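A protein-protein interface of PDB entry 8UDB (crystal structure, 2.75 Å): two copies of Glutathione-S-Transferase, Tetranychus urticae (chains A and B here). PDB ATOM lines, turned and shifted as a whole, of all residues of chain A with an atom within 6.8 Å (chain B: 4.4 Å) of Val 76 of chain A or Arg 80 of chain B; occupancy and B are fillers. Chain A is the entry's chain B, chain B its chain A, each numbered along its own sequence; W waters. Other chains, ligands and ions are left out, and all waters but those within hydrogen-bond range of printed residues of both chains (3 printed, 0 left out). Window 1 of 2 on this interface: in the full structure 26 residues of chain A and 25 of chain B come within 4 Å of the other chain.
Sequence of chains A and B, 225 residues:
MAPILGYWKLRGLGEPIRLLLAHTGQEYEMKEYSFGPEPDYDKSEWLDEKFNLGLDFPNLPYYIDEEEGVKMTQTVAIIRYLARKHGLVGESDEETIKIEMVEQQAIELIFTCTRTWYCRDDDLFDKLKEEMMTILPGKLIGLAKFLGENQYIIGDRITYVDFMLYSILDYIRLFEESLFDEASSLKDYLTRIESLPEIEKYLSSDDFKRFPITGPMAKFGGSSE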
ATOM      1  N   ILE A  17     -19.754 -14.744  14.776  1.00  0.00           N
ATOM      2  CA  ILE A  17     -20.429 -15.986  15.096  1.00  0.00           C
ATOM      3  C   ILE A  17     -20.367 -16.947  13.908  1.00  0.00           C
ATOM      4  O   ILE A  17     -20.138 -18.136  14.091  1.00  0.00           O
ATOM      5  CB  ILE A  17     -21.878 -15.737  15.537  1.00  0.00           C
ATOM      6  CG1 ILE A  17     -21.934 -14.896  16.812  1.00  0.00           C
ATOM      7  CG2 ILE A  17     -22.563 -17.080  15.709  1.00  0.00           C
ATOM      8  CD1 ILE A  17     -23.261 -14.208  17.060  1.00  0.00           C
ATOM      9  N   PRO A  61     -28.370 -10.193  16.765  1.00  0.00           N
ATOM     10  CA  PRO A  61     -28.707 -11.549  16.337  1.00  0.00           C
ATOM     11  C   PRO A  61     -29.323 -12.391  17.441  1.00  0.00           C
ATOM     12  O   PRO A  61     -29.286 -12.009  18.608  1.00  0.00           O
ATOM     13  CB  PRO A  61     -27.340 -12.126  15.954  1.00  0.00           C
ATOM     14  CG  PRO A  61     -26.395 -11.465  16.936  1.00  0.00           C
ATOM     15  CD  PRO A  61     -26.929 -10.052  17.037  1.00  0.00           C
ATOM     16  N   MET A  72     -31.278 -17.941  22.398  1.00  0.00           N
ATOM     17  CA  MET A  72     -30.535 -16.789  22.978  1.00  0.00           C
ATOM     18  C   MET A  72     -30.649 -15.546  22.095  1.00  0.00           C
ATOM     19  O   MET A  72     -31.058 -15.693  20.938  1.00  0.00           O
ATOM     20  CB  MET A  72     -29.056 -17.167  23.080  1.00  0.00           C
ATOM     21  CG  MET A  72     -28.794 -18.419  23.876  1.00  0.00           C
ATOM     22  SD  MET A  72     -27.033 -18.804  23.849  1.00  0.00           S
ATOM     23  CE  MET A  72     -26.418 -17.537  24.954  1.00  0.00           C
ATOM     24  N   GLN A  74     -28.053 -12.541  22.693  1.00  0.00           N
ATOM     25  CA  GLN A  74     -26.976 -11.532  22.909  1.00  0.00           C
ATOM     26  C   GLN A  74     -25.697 -12.003  22.206  1.00  0.00           C
ATOM     27  O   GLN A  74     -25.222 -13.092  22.546  1.00  0.00           O
ATOM     28  CB  GLN A  74     -26.785 -11.234  24.397  1.00  0.00           C
ATOM     29  CG  GLN A  74     -28.009 -10.643  25.084  1.00  0.00           C
ATOM     30  CD  GLN A  74     -28.412  -9.296  24.537  1.00  0.00           C
ATOM     31  OE1 GLN A  74     -27.622  -8.356  24.496  1.00  0.00           O
ATOM     32  NE2 GLN A  74     -29.659  -9.191  24.110  1.00  0.00           N
ATOM     33  N   THR A  75     -25.140 -11.195  21.303  1.00  0.00           N
ATOM     34  CA  THR A  75     -23.956 -11.599  20.490  1.00  0.00           C
ATOM     35  C   THR A  75     -22.855 -12.239  21.343  1.00  0.00           C
ATOM     36  O   THR A  75     -22.440 -13.357  21.003  1.00  0.00           O
ATOM     37  CB  THR A  75     -23.373 -10.396  19.737  1.00  0.00           C
ATOM     38  OG1 THR A  75     -24.434  -9.726  19.058  1.00  0.00           O
ATOM     39  CG2 THR A  75     -22.294 -10.783  18.751  1.00  0.00           C
ATOM     40  N   VAL A  76     -22.393 -11.551  22.387  1.00  0.00           N
ATOM     41  CA  VAL A  76     -21.265 -12.062  23.221  1.00  0.00           C
ATOM     42  C   VAL A  76     -21.707 -13.341  23.926  1.00  0.00           C
ATOM     43  O   VAL A  76     -20.910 -14.284  23.993  1.00  0.00           O
ATOM     44  CB  VAL A  76     -20.807 -10.990  24.224  1.00  0.00           C
ATOM     45  CG1 VAL A  76     -19.540 -11.396  24.955  1.00  0.00           C
ATOM     46  CG2 VAL A  76     -20.619  -9.655  23.534  1.00  0.00           C
ATOM     47  N   ALA A  77     -22.942 -13.365  24.411  1.00  0.00           N
ATOM     48  CA  ALA A  77     -23.471 -14.575  25.068  1.00  0.00           C
ATOM     49  C   ALA A  77     -23.546 -15.712  24.048  1.00  0.00           C
ATOM     50  O   ALA A  77     -23.200 -16.844  24.410  1.00  0.00           O
ATOM     51  CB  ALA A  77     -24.818 -14.262  25.652  1.00  0.00           C
ATOM     52  N   ILE A  78     -23.959 -15.408  22.817  1.00  0.00           N
ATOM     53  CA  ILE A  78     -24.116 -16.444  21.809  1.00  0.00           C
ATOM     54  C   ILE A  78     -22.745 -17.043  21.491  1.00  0.00           C
ATOM     55  O   ILE A  78     -22.562 -18.263  21.489  1.00  0.00           O
ATOM     56  CB  ILE A  78     -24.810 -15.895  20.545  1.00  0.00           C
ATOM     57  CG1 ILE A  78     -26.213 -15.366  20.837  1.00  0.00           C
ATOM     58  CG2 ILE A  78     -24.839 -16.952  19.453  1.00  0.00           C
ATOM     59  CD1 ILE A  78     -26.894 -14.743  19.643  1.00  0.00           C
ATOM     60  N   ILE A  79     -21.771 -16.164  21.237  1.00  0.00           N
ATOM     61  CA  ILE A  79     -20.485 -16.636  20.773  1.00  0.00           C
ATOM     62  C   ILE A  79     -19.760 -17.359  21.917  1.00  0.00           C
ATOM     63  O   ILE A  79     -19.108 -18.371  21.686  1.00  0.00           O
ATOM     64  CB  ILE A  79     -19.688 -15.485  20.133  1.00  0.00           C
ATOM     65  CG1 ILE A  79     -18.594 -16.015  19.204  1.00  0.00           C
ATOM     66  CG2 ILE A  79     -19.124 -14.529  21.177  1.00  0.00           C
ATOM     67  CD1 ILE A  79     -17.781 -14.927  18.540  1.00  0.00           C
ATOM     68  N   ARG A  80     -19.902 -16.881  23.157  1.00  0.00           N
ATOM     69  CA  ARG A  80     -19.287 -17.574  24.279  1.00  0.00           C
ATOM     70  C   ARG A  80     -19.913 -18.959  24.446  1.00  0.00           C
ATOM     71  O   ARG A  80     -19.213 -19.917  24.741  1.00  0.00           O
ATOM     72  CB  ARG A  80     -19.389 -16.752  25.564  1.00  0.00           C
ATOM     73  CG  ARG A  80     -18.416 -15.588  25.615  1.00  0.00           C
ATOM     74  CD  ARG A  80     -18.903 -14.461  26.501  1.00  0.00           C
ATOM     75  NE  ARG A  80     -18.918 -14.861  27.897  1.00  0.00           N
ATOM     76  CZ  ARG A  80     -17.841 -15.184  28.619  1.00  0.00           C
ATOM     77  NH1 ARG A  80     -16.621 -15.006  28.126  1.00  0.00           N
ATOM     78  NH2 ARG A  80     -17.994 -15.653  29.852  1.00  0.00           N
ATOM     79  N   TYR A  81     -21.226 -19.062  24.231  1.00  0.00           N
ATOM     80  CA  TYR A  81     -21.920 -20.337  24.331  1.00  0.00           C
ATOM     81  C   TYR A  81     -21.367 -21.324  23.297  1.00  0.00           C
ATOM     82  O   TYR A  81     -21.102 -22.496  23.601  1.00  0.00           O
ATOM     83  CB  TYR A  81     -23.438 -20.148  24.179  1.00  0.00           C
ATOM     84  CG  TYR A  81     -24.161 -21.413  23.790  1.00  0.00           C
ATOM     85  CD1 TYR A  81     -24.465 -22.384  24.733  1.00  0.00           C
ATOM     86  CD2 TYR A  81     -24.440 -21.691  22.455  1.00  0.00           C
ATOM     87  CE1 TYR A  81     -25.087 -23.567  24.363  1.00  0.00           C
ATOM     88  CE2 TYR A  81     -25.059 -22.873  22.072  1.00  0.00           C
ATOM     89  CZ  TYR A  81     -25.372 -23.818  23.030  1.00  0.00           C
ATOM     90  OH  TYR A  81     -25.953 -24.996  22.693  1.00  0.00           O
ATOM     91  N   ARG A  84     -17.757 -22.231  24.254  1.00  0.00           N
ATOM     92  CA  ARG A  84     -17.720 -23.215  25.324  1.00  0.00           C
ATOM     93  C   ARG A  84     -17.979 -24.600  24.744  1.00  0.00           C
ATOM     94  O   ARG A  84     -17.345 -25.561  25.156  1.00  0.00           O
ATOM     95  CB  ARG A  84     -18.727 -22.922  26.440  1.00  0.00           C
ATOM     96  CG  ARG A  84     -18.216 -22.017  27.549  1.00  0.00           C
ATOM     97  CD  ARG A  84     -19.247 -21.766  28.631  1.00  0.00           C
ATOM     98  NE  ARG A  84     -20.056 -20.578  28.364  1.00  0.00           N
ATOM     99  CZ  ARG A  84     -21.295 -20.602  27.904  1.00  0.00           C
ATOM    100  NH1 ARG A  84     -21.823 -21.743  27.502  1.00  0.00           N
ATOM    101  NH2 ARG A  84     -21.989 -19.488  27.779  1.00  0.00           N
ATOM    102  N   ASP A  93      -7.761 -19.793  34.356  1.00  0.00           N
ATOM    103  CA  ASP A  93      -8.293 -18.472  34.652  1.00  0.00           C
ATOM    104  C   ASP A  93      -7.349 -17.424  34.049  1.00  0.00           C
ATOM    105  O   ASP A  93      -7.785 -16.346  33.671  1.00  0.00           O
ATOM    106  CB  ASP A  93      -8.557 -18.228  36.146  1.00  0.00           C
ATOM    107  CG  ASP A  93      -9.359 -16.952  36.405  1.00  0.00           C
ATOM    108  OD1 ASP A  93     -10.352 -16.734  35.703  1.00  0.00           O
ATOM    109  OD2 ASP A  93      -8.995 -16.168  37.298  1.00  0.00           O
ATOM    110  N   THR A  96      -8.298 -16.995  30.472  1.00  0.00           N
ATOM    111  CA  THR A  96      -9.643 -16.451  30.400  1.00  0.00           C
ATOM    112  C   THR A  96      -9.610 -14.936  30.618  1.00  0.00           C
ATOM    113  O   THR A  96     -10.365 -14.228  29.974  1.00  0.00           O
ATOM    114  CB  THR A  96     -10.590 -17.183  31.371  1.00  0.00           C
ATOM    115  OG1 THR A  96     -10.678 -18.564  31.021  1.00  0.00           O
ATOM    116  CG2 THR A  96     -11.990 -16.602  31.375  1.00  0.00           C
ATOM    117  N   ILE A  99      -8.348 -13.320  27.380  1.00  0.00           N
ATOM    118  CA  ILE A  99      -9.386 -13.484  26.368  1.00  0.00           C
ATOM    119  C   ILE A  99     -10.509 -12.471  26.570  1.00  0.00           C
ATOM    120  O   ILE A  99     -10.967 -11.857  25.617  1.00  0.00           O
ATOM    121  CB  ILE A  99      -9.933 -14.923  26.394  1.00  0.00           C
ATOM    122  CG1 ILE A  99      -8.923 -15.900  25.797  1.00  0.00           C
ATOM    123  CG2 ILE A  99     -11.285 -15.028  25.707  1.00  0.00           C
ATOM    124  CD1 ILE A  99      -9.302 -17.345  25.954  1.00  0.00           C
ATOM    125  N   GLU A 100     -10.982 -12.325  27.809  1.00  0.00           N
ATOM    126  CA  GLU A 100     -12.150 -11.505  28.078  1.00  0.00           C
ATOM    127  C   GLU A 100     -11.770 -10.033  27.986  1.00  0.00           C
ATOM    128  O   GLU A 100     -12.614  -9.186  27.733  1.00  0.00           O
ATOM    129  CB  GLU A 100     -12.760 -11.917  29.413  1.00  0.00           C
ATOM    130  CG  GLU A 100     -13.307 -13.333  29.337  1.00  0.00           C
ATOM    131  CD  GLU A 100     -14.087 -13.863  30.526  1.00  0.00           C
ATOM    132  OE1 GLU A 100     -13.982 -13.279  31.633  1.00  0.00           O
ATOM    133  OE2 GLU A 100     -14.822 -14.843  30.326  1.00  0.00           O
ATOM    134  N   MET A 101     -10.490  -9.724  28.159  1.00  0.00           N
ATOM    135  CA  MET A 101     -10.026  -8.358  27.979  1.00  0.00           C
ATOM    136  C   MET A 101     -10.113  -7.997  26.497  1.00  0.00           C
ATOM    137  O   MET A 101     -10.624  -6.940  26.121  1.00  0.00           O
ATOM    138  CB  MET A 101      -8.595  -8.212  28.506  1.00  0.00           C
ATOM    139  CG  MET A 101      -8.567  -7.964  30.008  1.00  0.00           C
ATOM    140  SD  MET A 101      -7.042  -7.212  30.665  1.00  0.00           S
ATOM    141  CE  MET A 101      -5.823  -8.495  30.357  1.00  0.00           C
ATOM    142  N   GLU A 103     -11.873  -9.573  24.138  1.00  0.00           N
ATOM    143  CA  GLU A 103     -13.297  -9.562  23.853  1.00  0.00           C
ATOM    144  C   GLU A 103     -13.866  -8.165  24.041  1.00  0.00           C
ATOM    145  O   GLU A 103     -14.515  -7.635  23.143  1.00  0.00           O
ATOM    146  CB  GLU A 103     -14.019 -10.535  24.783  1.00  0.00           C
ATOM    147  CG  GLU A 103     -15.530 -10.421  24.726  1.00  0.00           C
ATOM    148  CD  GLU A 103     -16.226 -11.133  25.871  1.00  0.00           C
ATOM    149  OE1 GLU A 103     -16.228 -12.376  25.854  1.00  0.00           O
ATOM    150  OE2 GLU A 103     -16.725 -10.452  26.791  1.00  0.00           O
ATOM    151  N   GLN A 104     -13.624  -7.607  25.227  1.00  0.00           N
ATOM    152  CA  GLN A 104     -14.201  -6.341  25.632  1.00  0.00           C
ATOM    153  C   GLN A 104     -13.533  -5.168  24.923  1.00  0.00           C
ATOM    154  O   GLN A 104     -14.171  -4.151  24.677  1.00  0.00           O
ATOM    155  CB  GLN A 104     -14.118  -6.215  27.151  1.00  0.00           C
ATOM    156  CG  GLN A 104     -15.153  -7.083  27.862  1.00  0.00           C
ATOM    157  CD  GLN A 104     -16.554  -6.676  27.464  1.00  0.00           C
ATOM    158  OE1 GLN A 104     -16.913  -5.501  27.557  1.00  0.00           O
ATOM    159  NE2 GLN A 104     -17.325  -7.626  26.953  1.00  0.00           N
ATOM    160  N   ILE A 107     -15.290  -5.234  21.554  1.00  0.00           N
ATOM    161  CA  ILE A 107     -16.598  -4.621  21.684  1.00  0.00           C
ATOM    162  C   ILE A 107     -16.491  -3.113  21.870  1.00  0.00           C
ATOM    163  O   ILE A 107     -17.367  -2.408  21.404  1.00  0.00           O
ATOM    164  CB  ILE A 107     -17.380  -5.300  22.820  1.00  0.00           C
ATOM    165  CG1 ILE A 107     -17.933  -6.619  22.305  1.00  0.00           C
ATOM    166  CG2 ILE A 107     -18.492  -4.432  23.373  1.00  0.00           C
ATOM    167  CD1 ILE A 107     -18.211  -7.582  23.396  1.00  0.00           C
ATOM    168  N   TYR A 160     -12.267 -17.776  20.531  1.00  0.00           N
ATOM    169  CA  TYR A 160     -13.433 -17.118  19.883  1.00  0.00           C
ATOM    170  C   TYR A 160     -13.170 -15.625  19.672  1.00  0.00           C
ATOM    171  O   TYR A 160     -13.776 -15.042  18.764  1.00  0.00           O
ATOM    172  CB  TYR A 160     -14.703 -17.318  20.713  1.00  0.00           C
ATOM    173  CG  TYR A 160     -14.757 -16.567  22.019  1.00  0.00           C
ATOM    174  CD1 TYR A 160     -13.993 -16.959  23.103  1.00  0.00           C
ATOM    175  CD2 TYR A 160     -15.564 -15.452  22.164  1.00  0.00           C
ATOM    176  CE1 TYR A 160     -14.043 -16.273  24.305  1.00  0.00           C
ATOM    177  CE2 TYR A 160     -15.618 -14.750  23.355  1.00  0.00           C
ATOM    178  CZ  TYR A 160     -14.855 -15.162  24.430  1.00  0.00           C
ATOM    179  OH  TYR A 160     -14.899 -14.475  25.617  1.00  0.00           O
ATOM    180  N   MET A 164     -13.850 -12.381  16.682  1.00  0.00           N
ATOM    181  CA  MET A 164     -14.405 -11.092  17.043  1.00  0.00           C
ATOM    182  C   MET A 164     -13.469  -9.992  16.554  1.00  0.00           C
ATOM    183  O   MET A 164     -13.899  -8.977  15.984  1.00  0.00           O
ATOM    184  CB  MET A 164     -14.542 -11.000  18.563  1.00  0.00           C
ATOM    185  CG  MET A 164     -15.612 -11.913  19.109  1.00  0.00           C
ATOM    186  SD  MET A 164     -15.861 -11.568  20.845  1.00  0.00           S
ATOM    187  CE  MET A 164     -16.717 -10.002  20.729  1.00  0.00           C
ATOM    188  N   VAL B  76     -16.279  -5.617  32.350  1.00  0.00           N
ATOM    189  CA  VAL B  76     -16.937  -6.957  32.335  1.00  0.00           C
ATOM    190  C   VAL B  76     -15.904  -8.036  32.662  1.00  0.00           C
ATOM    191  O   VAL B  76     -16.247  -8.981  33.383  1.00  0.00           O
ATOM    192  CB  VAL B  76     -17.621  -7.221  30.982  1.00  0.00           C
ATOM    193  CG1 VAL B  76     -18.382  -8.536  30.974  1.00  0.00           C
ATOM    194  CG2 VAL B  76     -18.531  -6.074  30.596  1.00  0.00           C
ATOM    195  N   ALA B  77     -14.687  -7.886  32.149  1.00  0.00           N
ATOM    196  CA  ALA B  77     -13.615  -8.858  32.435  1.00  0.00           C
ATOM    197  C   ALA B  77     -13.258  -8.785  33.917  1.00  0.00           C
ATOM    198  O   ALA B  77     -12.934  -9.828  34.500  1.00  0.00           O
ATOM    199  CB  ALA B  77     -12.430  -8.552  31.563  1.00  0.00           C
ATOM    200  N   ILE B  78     -13.335  -7.591  34.500  1.00  0.00           N
ATOM    201  CA  ILE B  78     -12.962  -7.419  35.894  1.00  0.00           C
ATOM    202  C   ILE B  78     -14.013  -8.091  36.769  1.00  0.00           C
ATOM    203  O   ILE B  78     -13.688  -8.869  37.679  1.00  0.00           O
ATOM    204  CB  ILE B  78     -12.773  -5.928  36.239  1.00  0.00           C
ATOM    205  CG1 ILE B  78     -11.645  -5.290  35.422  1.00  0.00           C
ATOM    206  CG2 ILE B  78     -12.538  -5.750  37.726  1.00  0.00           C
ATOM    207  CD1 ILE B  78     -11.466  -3.813  35.670  1.00  0.00           C
ATOM    208  N   ILE B  79     -15.280  -7.802  36.468  1.00  0.00           N
ATOM    209  CA  ILE B  79     -16.351  -8.281  37.325  1.00  0.00           C
ATOM    210  C   ILE B  79     -16.481  -9.802  37.180  1.00  0.00           C
ATOM    211  O   ILE B  79     -16.718 -10.491  38.169  1.00  0.00           O
ATOM    212  CB  ILE B  79     -17.662  -7.496  37.080  1.00  0.00           C
ATOM    213  CG1 ILE B  79     -18.576  -7.581  38.307  1.00  0.00           C
ATOM    214  CG2 ILE B  79     -18.355  -7.928  35.796  1.00  0.00           C
ATOM    215  CD1 ILE B  79     -19.886  -6.851  38.168  1.00  0.00           C
ATOM    216  N   ARG B  80     -16.302 -10.332  35.961  1.00  0.00           N
ATOM    217  CA  ARG B  80     -16.398 -11.772  35.754  1.00  0.00           C
ATOM    218  C   ARG B  80     -15.280 -12.445  36.551  1.00  0.00           C
ATOM    219  O   ARG B  80     -15.504 -13.489  37.158  1.00  0.00           O
ATOM    220  CB  ARG B  80     -16.321 -12.176  34.273  1.00  0.00           C
ATOM    221  CG  ARG B  80     -17.582 -11.976  33.434  1.00  0.00           C
ATOM    222  CD  ARG B  80     -17.424 -12.658  32.062  1.00  0.00           C
ATOM    223  NE  ARG B  80     -18.279 -12.188  30.962  1.00  0.00           N
ATOM    224  CZ  ARG B  80     -17.892 -11.953  29.688  1.00  0.00           C
ATOM    225  NH1 ARG B  80     -16.618 -12.007  29.349  1.00  0.00           N
ATOM    226  NH2 ARG B  80     -18.773 -11.677  28.732  1.00  0.00           N
ATOM    227  N   TYR B  81     -14.080 -11.844  36.546  1.00  0.00           N
ATOM    228  CA  TYR B  81     -12.934 -12.379  37.271  1.00  0.00           C
ATOM    229  C   TYR B  81     -13.254 -12.463  38.766  1.00  0.00           C
ATOM    230  O   TYR B  81     -12.990 -13.466  39.404  1.00  0.00           O
ATOM    231  CB  TYR B  81     -11.684 -11.521  37.006  1.00  0.00           C
ATOM    232  CG  TYR B  81     -10.605 -11.689  38.042  1.00  0.00           C
ATOM    233  CD1 TYR B  81      -9.747 -12.769  38.006  1.00  0.00           C
ATOM    234  CD2 TYR B  81     -10.517 -10.836  39.129  1.00  0.00           C
ATOM    235  CE1 TYR B  81      -8.790 -12.965  38.986  1.00  0.00           C
ATOM    236  CE2 TYR B  81      -9.575 -11.020  40.128  1.00  0.00           C
ATOM    237  CZ  TYR B  81      -8.704 -12.088  40.049  1.00  0.00           C
ATOM    238  OH  TYR B  81      -7.769 -12.275  41.031  1.00  0.00           O
ATOM    239  N   LEU B  82     -13.800 -11.388  39.327  1.00  0.00           N
ATOM    240  CA  LEU B  82     -14.176 -11.343  40.730  1.00  0.00           C
ATOM    241  C   LEU B  82     -15.330 -12.299  41.032  1.00  0.00           C
ATOM    242  O   LEU B  82     -15.351 -12.923  42.097  1.00  0.00           O
ATOM    243  CB  LEU B  82     -14.558  -9.899  41.077  1.00  0.00           C
ATOM    244  CG  LEU B  82     -13.394  -8.910  41.127  1.00  0.00           C
ATOM    245  CD1 LEU B  82     -13.895  -7.509  41.435  1.00  0.00           C
ATOM    246  CD2 LEU B  82     -12.356  -9.334  42.156  1.00  0.00           C
ATOM    247  N   ALA B  83     -16.298 -12.380  40.105  1.00  0.00           N
ATOM    248  CA  ALA B  83     -17.423 -13.295  40.231  1.00  0.00           C
ATOM    249  C   ALA B  83     -16.914 -14.731  40.279  1.00  0.00           C
ATOM    250  O   ALA B  83     -17.361 -15.501  41.119  1.00  0.00           O
ATOM    251  CB  ALA B  83     -18.394 -13.108  39.083  1.00  0.00           C
ATOM    252  N   ARG B  84     -16.006 -15.081  39.355  1.00  0.00           N
ATOM    253  CA  ARG B  84     -15.469 -16.434  39.283  1.00  0.00           C
ATOM    254  C   ARG B  84     -14.768 -16.758  40.591  1.00  0.00           C
ATOM    255  O   ARG B  84     -14.899 -17.871  41.079  1.00  0.00           O
ATOM    256  CB  ARG B  84     -14.515 -16.659  38.104  1.00  0.00           C
ATOM    257  CG  ARG B  84     -15.217 -17.064  36.817  1.00  0.00           C
ATOM    258  CD  ARG B  84     -14.287 -17.384  35.668  1.00  0.00           C
ATOM    259  NE  ARG B  84     -13.154 -16.476  35.575  1.00  0.00           N
ATOM    260  CZ  ARG B  84     -13.103 -15.383  34.810  1.00  0.00           C
ATOM    261  NH1 ARG B  84     -14.169 -14.991  34.136  1.00  0.00           N
ATOM    262  NH2 ARG B  84     -11.984 -14.682  34.728  1.00  0.00           N
ATOM    263  N   GLU B 103     -26.297  -9.881  31.636  1.00  0.00           N
ATOM    264  CA  GLU B 103     -25.089  -9.076  31.578  1.00  0.00           C
ATOM    265  C   GLU B 103     -25.111  -8.156  30.360  1.00  0.00           C
ATOM    266  O   GLU B 103     -24.935  -6.951  30.488  1.00  0.00           O
ATOM    267  CB  GLU B 103     -23.875  -9.999  31.493  1.00  0.00           C
ATOM    268  CG  GLU B 103     -22.574  -9.281  31.149  1.00  0.00           C
ATOM    269  CD  GLU B 103     -21.450 -10.237  30.765  1.00  0.00           C
ATOM    270  OE1 GLU B 103     -21.181 -10.361  29.541  1.00  0.00           O
ATOM    271  OE2 GLU B 103     -20.858 -10.882  31.680  1.00  0.00           O
ATOM    272  N   GLN B 104     -25.309  -8.757  29.184  1.00  0.00           N
ATOM    273  CA  GLN B 104     -25.223  -8.078  27.905  1.00  0.00           C
ATOM    274  C   GLN B 104     -26.432  -7.173  27.691  1.00  0.00           C
ATOM    275  O   GLN B 104     -26.329  -6.140  27.037  1.00  0.00           O
ATOM    276  CB  GLN B 104     -25.088  -9.126  26.805  1.00  0.00           C
ATOM    277  CG  GLN B 104     -23.722  -9.810  26.784  1.00  0.00           C
ATOM    278  CD  GLN B 104     -22.650  -8.810  26.453  1.00  0.00           C
ATOM    279  OE1 GLN B 104     -22.777  -8.068  25.486  1.00  0.00           O
ATOM    280  NE2 GLN B 104     -21.637  -8.726  27.290  1.00  0.00           N
ATOM    281  N   TYR B 160     -23.294 -11.930  39.835  1.00  0.00           N
ATOM    282  CA  TYR B 160     -22.594 -10.637  39.620  1.00  0.00           C
ATOM    283  C   TYR B 160     -23.475  -9.688  38.816  1.00  0.00           C
ATOM    284  O   TYR B 160     -23.351  -8.469  38.972  1.00  0.00           O
ATOM    285  CB  TYR B 160     -21.253 -10.842  38.911  1.00  0.00           C
ATOM    286  CG  TYR B 160     -21.304 -11.335  37.488  1.00  0.00           C
ATOM    287  CD1 TYR B 160     -21.558 -12.664  37.196  1.00  0.00           C
ATOM    288  CD2 TYR B 160     -21.087 -10.471  36.429  1.00  0.00           C
ATOM    289  CE1 TYR B 160     -21.592 -13.121  35.890  1.00  0.00           C
ATOM    290  CE2 TYR B 160     -21.126 -10.909  35.117  1.00  0.00           C
ATOM    291  CZ  TYR B 160     -21.379 -12.240  34.845  1.00  0.00           C
ATOM    292  OH  TYR B 160     -21.419 -12.685  33.548  1.00  0.00           O
HETATM  293  O   HOH W   1     -20.268  -6.281  25.875  1.00  0.00           O
HETATM  294  O   HOH W   2     -15.846  -4.072  29.878  1.00  0.00           O
HETATM  295  O   HOH W   3     -23.723  -9.204  23.444  1.00  0.00           O
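OE2 of Glu 103 of chain A is in salt-bridge range of NH1 of Arg 80 of chain B, 3.0 Å away. OE2 of Glu 100 of chain A lies within salt-bridge range of NH1 of Arg 80 of chain B. The guanidinium group (NH1) of Arg 80 of chain B lies close to the guanidinium group (NH1) of Arg 80 of chain A. The guanidinium group (NH1) of Arg 84 of chain B is in salt-bridge range of the side-chain carboxylate (OE1) of Glu 100 of chain A (3.0 Å). The guanidinium group of Arg 84 of chain B is in salt-bridge range of the side-chain carboxylate of Asp 93 of chain A, 2.8 Å away.
Of chain B, only Arg 80 and Gln 104 come within 4 Å of Val 76 of chain A. Arg 80 of chain B touches just these residues of chain A: Val 76, Arg 80, Glu 100 and Glu 103. Printed residues of chain B within 4 Å of Gln 104 of chain A: Val 76. Of the printed residues of chain A, Arg 84 of chain B touches Asp 93 (2.8 Å), Thr 96 (3.8 Å) and Glu 100 (3.0 Å). The nearest printed residue of chain B that does not touch Val 76 of chain A is Glu 103 of chain B (5.0 Å). The nearest residue of chain A that does not touch Arg 80 of chain B is Gln 104 of chain A (4.7 Å).
Of the 12 printed residues of chain B, 6 touch a printed residue of chain A. Hydrophobic or aromatic side chains of chain B that line the printed part of chain A: Val 76, Ala 77 and Tyr 81. Among the printed residues, Asp or Glu carboxylates within 4 Å of a Lys or Arg side-chain nitrogen of the other chain: Asp 93 of chain A with Arg 84 of chain B (2.8 Å), Glu 100 of chain A with Arg 80 of chain B (3.5 Å), Glu 100 of chain A with Arg 84 of chain B (3.0 Å) and Glu 103 of chain A with Arg 80 of chain B (3.0 Å).
Water W3 lies within hydrogen-bond range of OE1 of Gln 104 of chain B, N of Val 76 of chain A and N of Thr 75 of chain A. Water W2 lies within hydrogen-bond range of the side-chain amide oxygen (OE1) of Gln 104 of chain A and the backbone NH (N) of Val 76 of chain B. Water W1 bridges OE1 of Gln 104 of chain B (3.1 Å) and NE2 of Gln 104 of chain A (3.4 Å).
Val 76 of chain A touches Arg 80 of chain B, but with the chains exchanged Arg 80 of chain A does not touch Val 76 of chain B (7.1 Å). Val 76 of chain A touches Gln 104 of chain B, and with the chains exchanged Gln 104 of chain A touches Val 76 of chain B. Glu 103 of chain A touches Arg 80 of chain B, but with the chains exchanged Arg 80 of chain A does not touch Glu 103 of chain B (5.3 Å). Positions printed for both chains: 76, 77, 78, 79, 80, 81, 84, 103, 104 and 160. Of the 12 pairs that touch across the chains among the printed residues, 3 have their exchanged pair printed and touching as well.
NH2 of Arg 80 of chain B is in salt-bridge range of OE1 of Glu 103 of chain B (2.9 Å). OE1 of Glu 103 of chain B lies within hydrogen-bond range of NE2 of Gln 104 of chain B. OE2 of Glu 103 of chain A lies within hydrogen-bond range of NE2 of Gln 104 of chain A, at 2.9 Å. The side-chain carboxylate of Glu 100 of chain A is in salt-bridge range of the guanidinium group of Arg 80 of chain A, at 2.8 Å. The side-chain hydroxyl of Tyr 160 of chain A is in hydrogen-bond range of the side-chain carboxylate of Glu 103 of chain A (2.5 Å).
Among the printed residues, pairs that only touch across the chains: Val 76 of chain A with Gln 104 of chain B (3.3 Å), Gln 104 of chain A with Val 76 of chain B (3.5 Å), Gln 74 of chain A with Gln 104 of chain B (3.5 Å), Asp 93 of chain A with Tyr 81 of chain B (3.6 Å), Thr 96 of chain A with Arg 84 of chain B (3.8 Å), Val 76 of chain A with Arg 80 of chain B (3.9 Å) and Glu 100 of chain A with Ala 77 of chain B (3.9 Å).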
